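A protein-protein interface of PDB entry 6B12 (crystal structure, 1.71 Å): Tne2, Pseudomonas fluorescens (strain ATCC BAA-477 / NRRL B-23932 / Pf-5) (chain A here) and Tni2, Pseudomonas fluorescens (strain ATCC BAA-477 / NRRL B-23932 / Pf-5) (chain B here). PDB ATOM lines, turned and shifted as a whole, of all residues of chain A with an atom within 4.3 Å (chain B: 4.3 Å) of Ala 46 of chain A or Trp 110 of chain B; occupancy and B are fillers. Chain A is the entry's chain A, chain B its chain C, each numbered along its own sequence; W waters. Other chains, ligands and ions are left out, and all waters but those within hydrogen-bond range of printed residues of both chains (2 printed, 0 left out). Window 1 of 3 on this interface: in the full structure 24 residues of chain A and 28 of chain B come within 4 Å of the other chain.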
ATOM      1  N   GLY A  42      22.925 -24.836  -1.154  1.00  0.00           N
ATOM      2  CA  GLY A  42      23.108 -24.261   0.168  1.00  0.00           C
ATOM      3  C   GLY A  42      24.573 -24.130   0.522  1.00  0.00           C
ATOM      4  O   GLY A  42      24.967 -23.244   1.286  1.00  0.00           O
ATOM      5  N   GLN A  43      25.385 -25.036   0.003  1.00  0.00           N
ATOM      6  CA  GLN A  43      26.826 -24.946   0.166  1.00  0.00           C
ATOM      7  C   GLN A  43      27.355 -23.643  -0.430  1.00  0.00           C
ATOM      8  O   GLN A  43      28.158 -22.933   0.196  1.00  0.00           O
ATOM      9  CB  GLN A  43      27.452 -26.165  -0.506  1.00  0.00           C
ATOM     10  CG  GLN A  43      28.876 -26.407  -0.156  1.00  0.00           C
ATOM     11  CD  GLN A  43      29.411 -27.654  -0.807  1.00  0.00           C
ATOM     12  OE1 GLN A  43      28.728 -28.297  -1.603  1.00  0.00           O
ATOM     13  NE2 GLN A  43      30.664 -27.983  -0.509  1.00  0.00           N
ATOM     14  N   ALA A  44      26.934 -23.320  -1.658  1.00  0.00           N
ATOM     15  CA  ALA A  44      27.413 -22.082  -2.278  1.00  0.00           C
ATOM     16  C   ALA A  44      26.892 -20.864  -1.530  1.00  0.00           C
ATOM     17  O   ALA A  44      27.604 -19.860  -1.394  1.00  0.00           O
ATOM     18  CB  ALA A  44      27.005 -22.026  -3.749  1.00  0.00           C
ATOM     19  N   GLU A  45      25.648 -20.930  -1.042  1.00  0.00           N
ATOM     20  CA  GLU A  45      25.124 -19.851  -0.207  1.00  0.00           C
ATOM     21  C   GLU A  45      25.979 -19.651   1.039  1.00  0.00           C
ATOM     22  O   GLU A  45      26.256 -18.510   1.426  1.00  0.00           O
ATOM     23  CB  GLU A  45      23.675 -20.134   0.177  1.00  0.00           C
ATOM     24  CG  GLU A  45      22.736 -20.066  -1.056  1.00  0.00           C
ATOM     25  CD  GLU A  45      21.328 -20.665  -0.834  1.00  0.00           C
ATOM     26  OE1 GLU A  45      21.066 -21.286   0.218  1.00  0.00           O
ATOM     27  OE2 GLU A  45      20.482 -20.521  -1.749  1.00  0.00           O
ATOM     28  N   ALA A  46      26.406 -20.743   1.689  1.00  0.00           N
ATOM     29  CA  ALA A  46      27.236 -20.585   2.883  1.00  0.00           C
ATOM     30  C   ALA A  46      28.575 -19.970   2.523  1.00  0.00           C
ATOM     31  O   ALA A  46      29.080 -19.098   3.236  1.00  0.00           O
ATOM     32  CB  ALA A  46      27.451 -21.931   3.591  1.00  0.00           C
ATOM     33  N   ILE A  47      29.146 -20.403   1.401  1.00  0.00           N
ATOM     34  CA  ILE A  47      30.420 -19.853   0.947  1.00  0.00           C
ATOM     35  C   ILE A  47      30.297 -18.354   0.718  1.00  0.00           C
ATOM     36  O   ILE A  47      31.150 -17.570   1.154  1.00  0.00           O
ATOM     37  CB  ILE A  47      30.872 -20.578  -0.327  1.00  0.00           C
ATOM     38  CG1 ILE A  47      31.323 -22.004   0.037  1.00  0.00           C
ATOM     39  CG2 ILE A  47      31.969 -19.778  -1.026  1.00  0.00           C
ATOM     40  CD1 ILE A  47      31.557 -22.881  -1.172  1.00  0.00           C
ATOM     41  N   MET A  48      29.231 -17.938   0.037  1.00  0.00           N
ATOM     42  CA  MET A  48      28.996 -16.515  -0.191  1.00  0.00           C
ATOM     43  C   MET A  48      28.805 -15.742   1.113  1.00  0.00           C
ATOM     44  O   MET A  48      28.986 -14.520   1.133  1.00  0.00           O
ATOM     45  CB  MET A  48      27.782 -16.308  -1.101  1.00  0.00           C
ATOM     46  CG  MET A  48      28.069 -16.507  -2.581  1.00  0.00           C
ATOM     47  SD  MET A  48      29.624 -15.517  -3.232  1.00  0.00           S
ATOM     48  CE  MET A  48      28.982 -13.685  -3.001  1.00  0.00           C
ATOM     49  N   GLN A  49      28.436 -16.454   2.184  1.00  0.00           N
ATOM     50  CA  GLN A  49      28.261 -15.875   3.512  1.00  0.00           C
ATOM     51  C   GLN A  49      29.458 -16.130   4.424  1.00  0.00           C
ATOM     52  O   GLN A  49      29.326 -16.105   5.656  1.00  0.00           O
ATOM     53  CB  GLN A  49      26.962 -16.387   4.139  1.00  0.00           C
ATOM     54  CG  GLN A  49      25.727 -15.867   3.401  1.00  0.00           C
ATOM     55  CD  GLN A  49      24.440 -16.513   3.896  1.00  0.00           C
ATOM     56  OE1 GLN A  49      23.810 -16.029   4.832  1.00  0.00           O
ATOM     57  NE2 GLN A  49      24.072 -17.634   3.290  1.00  0.00           N
ATOM     58  N   GLY A  50      30.636 -16.309   3.834  1.00  0.00           N
ATOM     59  CA  GLY A  50      31.867 -16.351   4.601  1.00  0.00           C
ATOM     60  C   GLY A  50      32.135 -17.634   5.350  1.00  0.00           C
ATOM     61  O   GLY A  50      32.991 -17.648   6.246  1.00  0.00           O
ATOM     62  N   LYS A  51      31.422 -18.740   5.011  1.00  0.00           N
ATOM     63  CA  LYS A  51      31.699 -19.990   5.721  1.00  0.00           C
ATOM     64  C   LYS A  51      32.613 -20.882   4.895  1.00  0.00           C
ATOM     65  O   LYS A  51      32.512 -20.914   3.668  1.00  0.00           O
ATOM     66  CB  LYS A  51      30.410 -20.766   6.028  1.00  0.00           C
ATOM     67  CG  LYS A  51      29.505 -20.107   7.077  1.00  0.00           C
ATOM     68  CD  LYS A  51      30.056 -20.264   8.501  1.00  0.00           C
ATOM     69  CE  LYS A  51      29.994 -21.751   8.971  1.00  0.00           C
ATOM     70  NZ  LYS A  51      30.456 -21.877  10.389  1.00  0.00           N
ATOM     71  N   ALA A  53      32.637 -23.818   3.692  1.00  0.00           N
ATOM     72  CA  ALA A  53      31.701 -24.919   3.481  1.00  0.00           C
ATOM     73  C   ALA A  53      32.236 -25.832   2.386  1.00  0.00           C
ATOM     74  O   ALA A  53      31.679 -25.950   1.295  1.00  0.00           O
ATOM     75  CB  ALA A  53      30.321 -24.361   3.135  1.00  0.00           C
ATOM     76  N   PHE A  54      33.356 -26.488   2.711  1.00  0.00           N
ATOM     77  CA  PHE A  54      34.067 -27.337   1.767  1.00  0.00           C
ATOM     78  C   PHE A  54      33.658 -28.797   1.903  1.00  0.00           C
ATOM     79  O   PHE A  54      33.555 -29.327   3.012  1.00  0.00           O
ATOM     80  CB  PHE A  54      35.572 -27.205   1.993  1.00  0.00           C
ATOM     81  CG  PHE A  54      36.056 -25.796   1.898  1.00  0.00           C
ATOM     82  CD1 PHE A  54      35.734 -25.019   0.792  1.00  0.00           C
ATOM     83  CD2 PHE A  54      36.777 -25.224   2.928  1.00  0.00           C
ATOM     84  CE1 PHE A  54      36.159 -23.699   0.701  1.00  0.00           C
ATOM     85  CE2 PHE A  54      37.210 -23.895   2.840  1.00  0.00           C
ATOM     86  CZ  PHE A  54      36.896 -23.139   1.729  1.00  0.00           C
ATOM     87  N   LEU B  55      25.167 -18.251  10.208  1.00  0.00           N
ATOM     88  CA  LEU B  55      24.471 -18.694   9.013  1.00  0.00           C
ATOM     89  C   LEU B  55      23.044 -18.936   9.457  1.00  0.00           C
ATOM     90  O   LEU B  55      22.825 -19.715  10.387  1.00  0.00           O
ATOM     91  CB  LEU B  55      25.128 -19.963   8.451  1.00  0.00           C
ATOM     92  CG  LEU B  55      24.749 -20.502   7.082  1.00  0.00           C
ATOM     93  CD1 LEU B  55      25.048 -19.486   5.951  1.00  0.00           C
ATOM     94  CD2 LEU B  55      25.525 -21.790   6.857  1.00  0.00           C
ATOM     95  N   LEU B  68      23.249 -21.202  12.588  1.00  0.00           N
ATOM     96  CA  LEU B  68      24.568 -21.793  12.821  1.00  0.00           C
ATOM     97  C   LEU B  68      25.487 -20.667  13.278  1.00  0.00           C
ATOM     98  O   LEU B  68      25.796 -19.756  12.504  1.00  0.00           O
ATOM     99  CB  LEU B  68      25.074 -22.463  11.555  1.00  0.00           C
ATOM    100  CG  LEU B  68      26.389 -23.208  11.726  1.00  0.00           C
ATOM    101  CD1 LEU B  68      26.295 -24.296  12.806  1.00  0.00           C
ATOM    102  CD2 LEU B  68      26.740 -23.788  10.374  1.00  0.00           C
ATOM    103  N   TYR B 108      28.443 -28.826  12.729  1.00  0.00           N
ATOM    104  CA  TYR B 108      27.523 -28.423  11.672  1.00  0.00           C
ATOM    105  C   TYR B 108      28.169 -27.351  10.795  1.00  0.00           C
ATOM    106  O   TYR B 108      28.839 -26.441  11.298  1.00  0.00           O
ATOM    107  CB  TYR B 108      26.218 -27.914  12.274  1.00  0.00           C
ATOM    108  CG  TYR B 108      25.389 -29.035  12.864  1.00  0.00           C
ATOM    109  CD1 TYR B 108      24.799 -29.990  12.039  1.00  0.00           C
ATOM    110  CD2 TYR B 108      25.216 -29.154  14.233  1.00  0.00           C
ATOM    111  CE1 TYR B 108      24.025 -31.040  12.571  1.00  0.00           C
ATOM    112  CE2 TYR B 108      24.426 -30.211  14.786  1.00  0.00           C
ATOM    113  CZ  TYR B 108      23.842 -31.133  13.930  1.00  0.00           C
ATOM    114  OH  TYR B 108      23.081 -32.169  14.430  1.00  0.00           O
ATOM    115  N   SER B 109      27.971 -27.470   9.475  1.00  0.00           N
ATOM    116  CA  SER B 109      28.778 -26.760   8.495  1.00  0.00           C
ATOM    117  C   SER B 109      27.984 -25.893   7.537  1.00  0.00           C
ATOM    118  O   SER B 109      28.442 -24.802   7.228  1.00  0.00           O
ATOM    119  CB  SER B 109      29.643 -27.740   7.705  1.00  0.00           C
ATOM    120  OG  SER B 109      30.497 -28.407   8.619  1.00  0.00           O
ATOM    121  N   TRP B 110      26.810 -26.331   7.065  1.00  0.00           N
ATOM    122  CA  TRP B 110      25.994 -25.488   6.189  1.00  0.00           C
ATOM    123  C   TRP B 110      24.627 -26.145   6.049  1.00  0.00           C
ATOM    124  O   TRP B 110      24.428 -27.282   6.478  1.00  0.00           O
ATOM    125  CB  TRP B 110      26.646 -25.269   4.816  1.00  0.00           C
ATOM    126  CG  TRP B 110      26.717 -26.462   3.856  1.00  0.00           C
ATOM    127  CD1 TRP B 110      25.746 -26.885   2.991  1.00  0.00           C
ATOM    128  CD2 TRP B 110      27.838 -27.331   3.648  1.00  0.00           C
ATOM    129  NE1 TRP B 110      26.180 -27.974   2.276  1.00  0.00           N
ATOM    130  CE2 TRP B 110      27.471 -28.259   2.650  1.00  0.00           C
ATOM    131  CE3 TRP B 110      29.116 -27.411   4.204  1.00  0.00           C
ATOM    132  CZ2 TRP B 110      28.327 -29.264   2.219  1.00  0.00           C
ATOM    133  CZ3 TRP B 110      29.974 -28.404   3.760  1.00  0.00           C
ATOM    134  CH2 TRP B 110      29.574 -29.319   2.785  1.00  0.00           C
ATOM    135  N   PHE B 111      23.688 -25.423   5.432  1.00  0.00           N
ATOM    136  CA  PHE B 111      22.311 -25.899   5.295  1.00  0.00           C
ATOM    137  C   PHE B 111      22.033 -26.314   3.857  1.00  0.00           C
ATOM    138  O   PHE B 111      22.602 -25.759   2.916  1.00  0.00           O
ATOM    139  CB  PHE B 111      21.295 -24.807   5.679  1.00  0.00           C
ATOM    140  CG  PHE B 111      21.373 -24.372   7.107  1.00  0.00           C
ATOM    141  CD1 PHE B 111      20.875 -25.176   8.124  1.00  0.00           C
ATOM    142  CD2 PHE B 111      21.959 -23.150   7.443  1.00  0.00           C
ATOM    143  CE1 PHE B 111      20.956 -24.776   9.453  1.00  0.00           C
ATOM    144  CE2 PHE B 111      22.035 -22.746   8.761  1.00  0.00           C
ATOM    145  CZ  PHE B 111      21.529 -23.542   9.772  1.00  0.00           C
ATOM    146  N   GLU B 112      21.139 -27.289   3.693  1.00  0.00           N
ATOM    147  CA  GLU B 112      20.577 -27.612   2.385  1.00  0.00           C
ATOM    148  C   GLU B 112      19.088 -27.823   2.549  1.00  0.00           C
ATOM    149  O   GLU B 112      18.592 -28.024   3.656  1.00  0.00           O
ATOM    150  CB  GLU B 112      21.192 -28.872   1.763  1.00  0.00           C
ATOM    151  CG  GLU B 112      22.682 -28.787   1.507  1.00  0.00           C
ATOM    152  CD  GLU B 112      23.046 -27.920   0.304  1.00  0.00           C
ATOM    153  OE1 GLU B 112      22.147 -27.460  -0.443  1.00  0.00           O
ATOM    154  OE2 GLU B 112      24.256 -27.696   0.131  1.00  0.00           O
ATOM    155  N   CYS B 124      20.840 -29.836   8.020  1.00  0.00           N
ATOM    156  CA  CYS B 124      22.138 -29.214   8.225  1.00  0.00           C
ATOM    157  C   CYS B 124      23.202 -30.276   8.003  1.00  0.00           C
ATOM    158  O   CYS B 124      23.030 -31.443   8.401  1.00  0.00           O
ATOM    159  CB  CYS B 124      22.238 -28.597   9.618  1.00  0.00           C
ATOM    160  SG  CYS B 124      23.649 -27.478   9.853  1.00  0.00           S
ATOM    161  N   MET B 125      24.259 -29.877   7.308  1.00  0.00           N
ATOM    162  CA  MET B 125      25.323 -30.799   6.929  1.00  0.00           C
ATOM    163  C   MET B 125      26.336 -30.833   8.064  1.00  0.00           C
ATOM    164  O   MET B 125      26.775 -29.794   8.536  1.00  0.00           O
ATOM    165  CB  MET B 125      25.953 -30.357   5.602  1.00  0.00           C
ATOM    166  CG  MET B 125      24.944 -30.186   4.481  1.00  0.00           C
ATOM    167  SD  MET B 125      23.886 -31.807   4.139  1.00  0.00           S
ATOM    168  CE  MET B 125      25.415 -32.903   3.794  1.00  0.00           C
ATOM    169  N   MET B 134      30.990 -36.382   5.788  1.00  0.00           N
ATOM    170  CA  MET B 134      29.819 -35.511   5.812  1.00  0.00           C
ATOM    171  C   MET B 134      28.565 -36.331   6.024  1.00  0.00           C
ATOM    172  O   MET B 134      28.396 -37.409   5.428  1.00  0.00           O
ATOM    173  CB  MET B 134      29.673 -34.715   4.507  1.00  0.00           C
ATOM    174  CG  MET B 134      30.867 -33.845   4.134  1.00  0.00           C
ATOM    175  SD  MET B 134      31.227 -32.485   5.493  1.00  0.00           S
ATOM    176  CE  MET B 134      29.413 -31.839   5.803  1.00  0.00           C
HETATM  177  O   HOH W   1      23.872 -22.919   3.836  1.00  0.00           O
HETATM  178  O   HOH W   2      30.842 -24.539  10.876  1.00  0.00           O
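The backbone NH (N) of Gly 42 of chain A is in hydrogen-bond range of the side-chain carboxylate (OE1) of Glu 112 of chain B (2.8 Å). N of Gln 43 of chain A is in hydrogen-bond range of OE2 of Glu 112 of chain B.
The backbone carbonyl oxygen (O) of Trp 110 of chain B lies within hydrogen-bond range of the backbone NH (N) of Met 125 of chain B (2.7 Å). The backbone NH of Ser 109 of chain B lies within hydrogen-bond range of the backbone carbonyl oxygen of Met 125 of chain B. The indole nitrogen (NE1) of Trp 110 of chain B sits at hydrogen-bond distance from the side-chain carboxylate (OE2) of Glu 112 of chain B. The backbone carbonyl oxygen of Glu 45 of chain A lies within hydrogen-bond range of the side-chain amide nitrogen of Gln 49 of chain A (3.0 Å). The backbone carbonyl oxygen (O) of Leu 55 of chain B lies within hydrogen-bond range of the backbone NH (N) of Leu 68 of chain B (2.7 Å). NE2 of Gln 43 of chain A lies within hydrogen-bond range of O of Ala 53 of chain A, at 2.9 Å.
Gly 42 of chain A touches Trp 110 of chain B (C to CD1, 3.9 Å). Gly 42 of chain A touches Phe 111 of chain B (CA to O, 3.2 Å). N of Gln 43 of chain A touches CD1 of Trp 110 of chain B, 3.5 Å away. Ala 46 of chain A touches Leu 55 of chain B. CB of Trp 110 of chain B touches CB of Ala 46 of chain A, 3.6 Å away. Leu 55 of chain B touches Gln 49 of chain A. Ser 109 of chain B touches Lys 51 of chain A. CB of Ala 53 of chain A touches CE3 of Trp 110 of chain B, 3.4 Å away. Phe 54 of chain A touches Trp 110 of chain B (O to CZ3, 3.8 Å).
Printed residues of chain B within 4 Å of Ala 46 of chain A: Leu 55 and Trp 110. Of the printed residues of chain B, Gln 49 of chain A touches Leu 55. Printed residues of chain B within 4 Å of Ala 53 of chain A: Trp 110. Of the printed residues of chain B, Phe 54 of chain A touches Trp 110 (3.8 Å). Of the printed residues of chain A, Leu 55 of chain B touches Ala 46 and Gln 49. Printed residues of chain A within 4 Å of Ser 109 of chain B: Lys 51 (3.8 Å). Trp 110 of chain B touches five residues of chain A. The nearest printed residue of chain A that does not touch Leu 55 of chain B is Lys 51 of chain A (4.3 Å).
Hydrophobic or aromatic side chains of chain A that line the printed part of chain B: Ala 46 and Ala 53. Of the 10 printed residues of chain B, 5 touch a printed residue of chain A. Printed residues of chain B that touch a printed residue of chain A: Leu 55, Ser 109, Trp 110, Phe 111 and Glu 112. Hydrophobic or aromatic side chains of chain B within 4 Å of the printed part of chain A: Leu 55 and Trp 110. Among the printed residues, no Asp or Glu carboxylate lies within 4 Å of a Lys or Arg side-chain nitrogen of the other chain.
Water W2 bridges the side-chain amino group (NZ) of Lys 51 of chain A (2.7 Å) and the backbone carbonyl oxygen (O) of Tyr 108 of chain B (2.8 Å). Water W1 bridges the backbone carbonyl oxygen (O) of Gly 42 of chain A (2.8 Å) and the backbone NH (N) of Phe 111 of chain B (3.0 Å).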
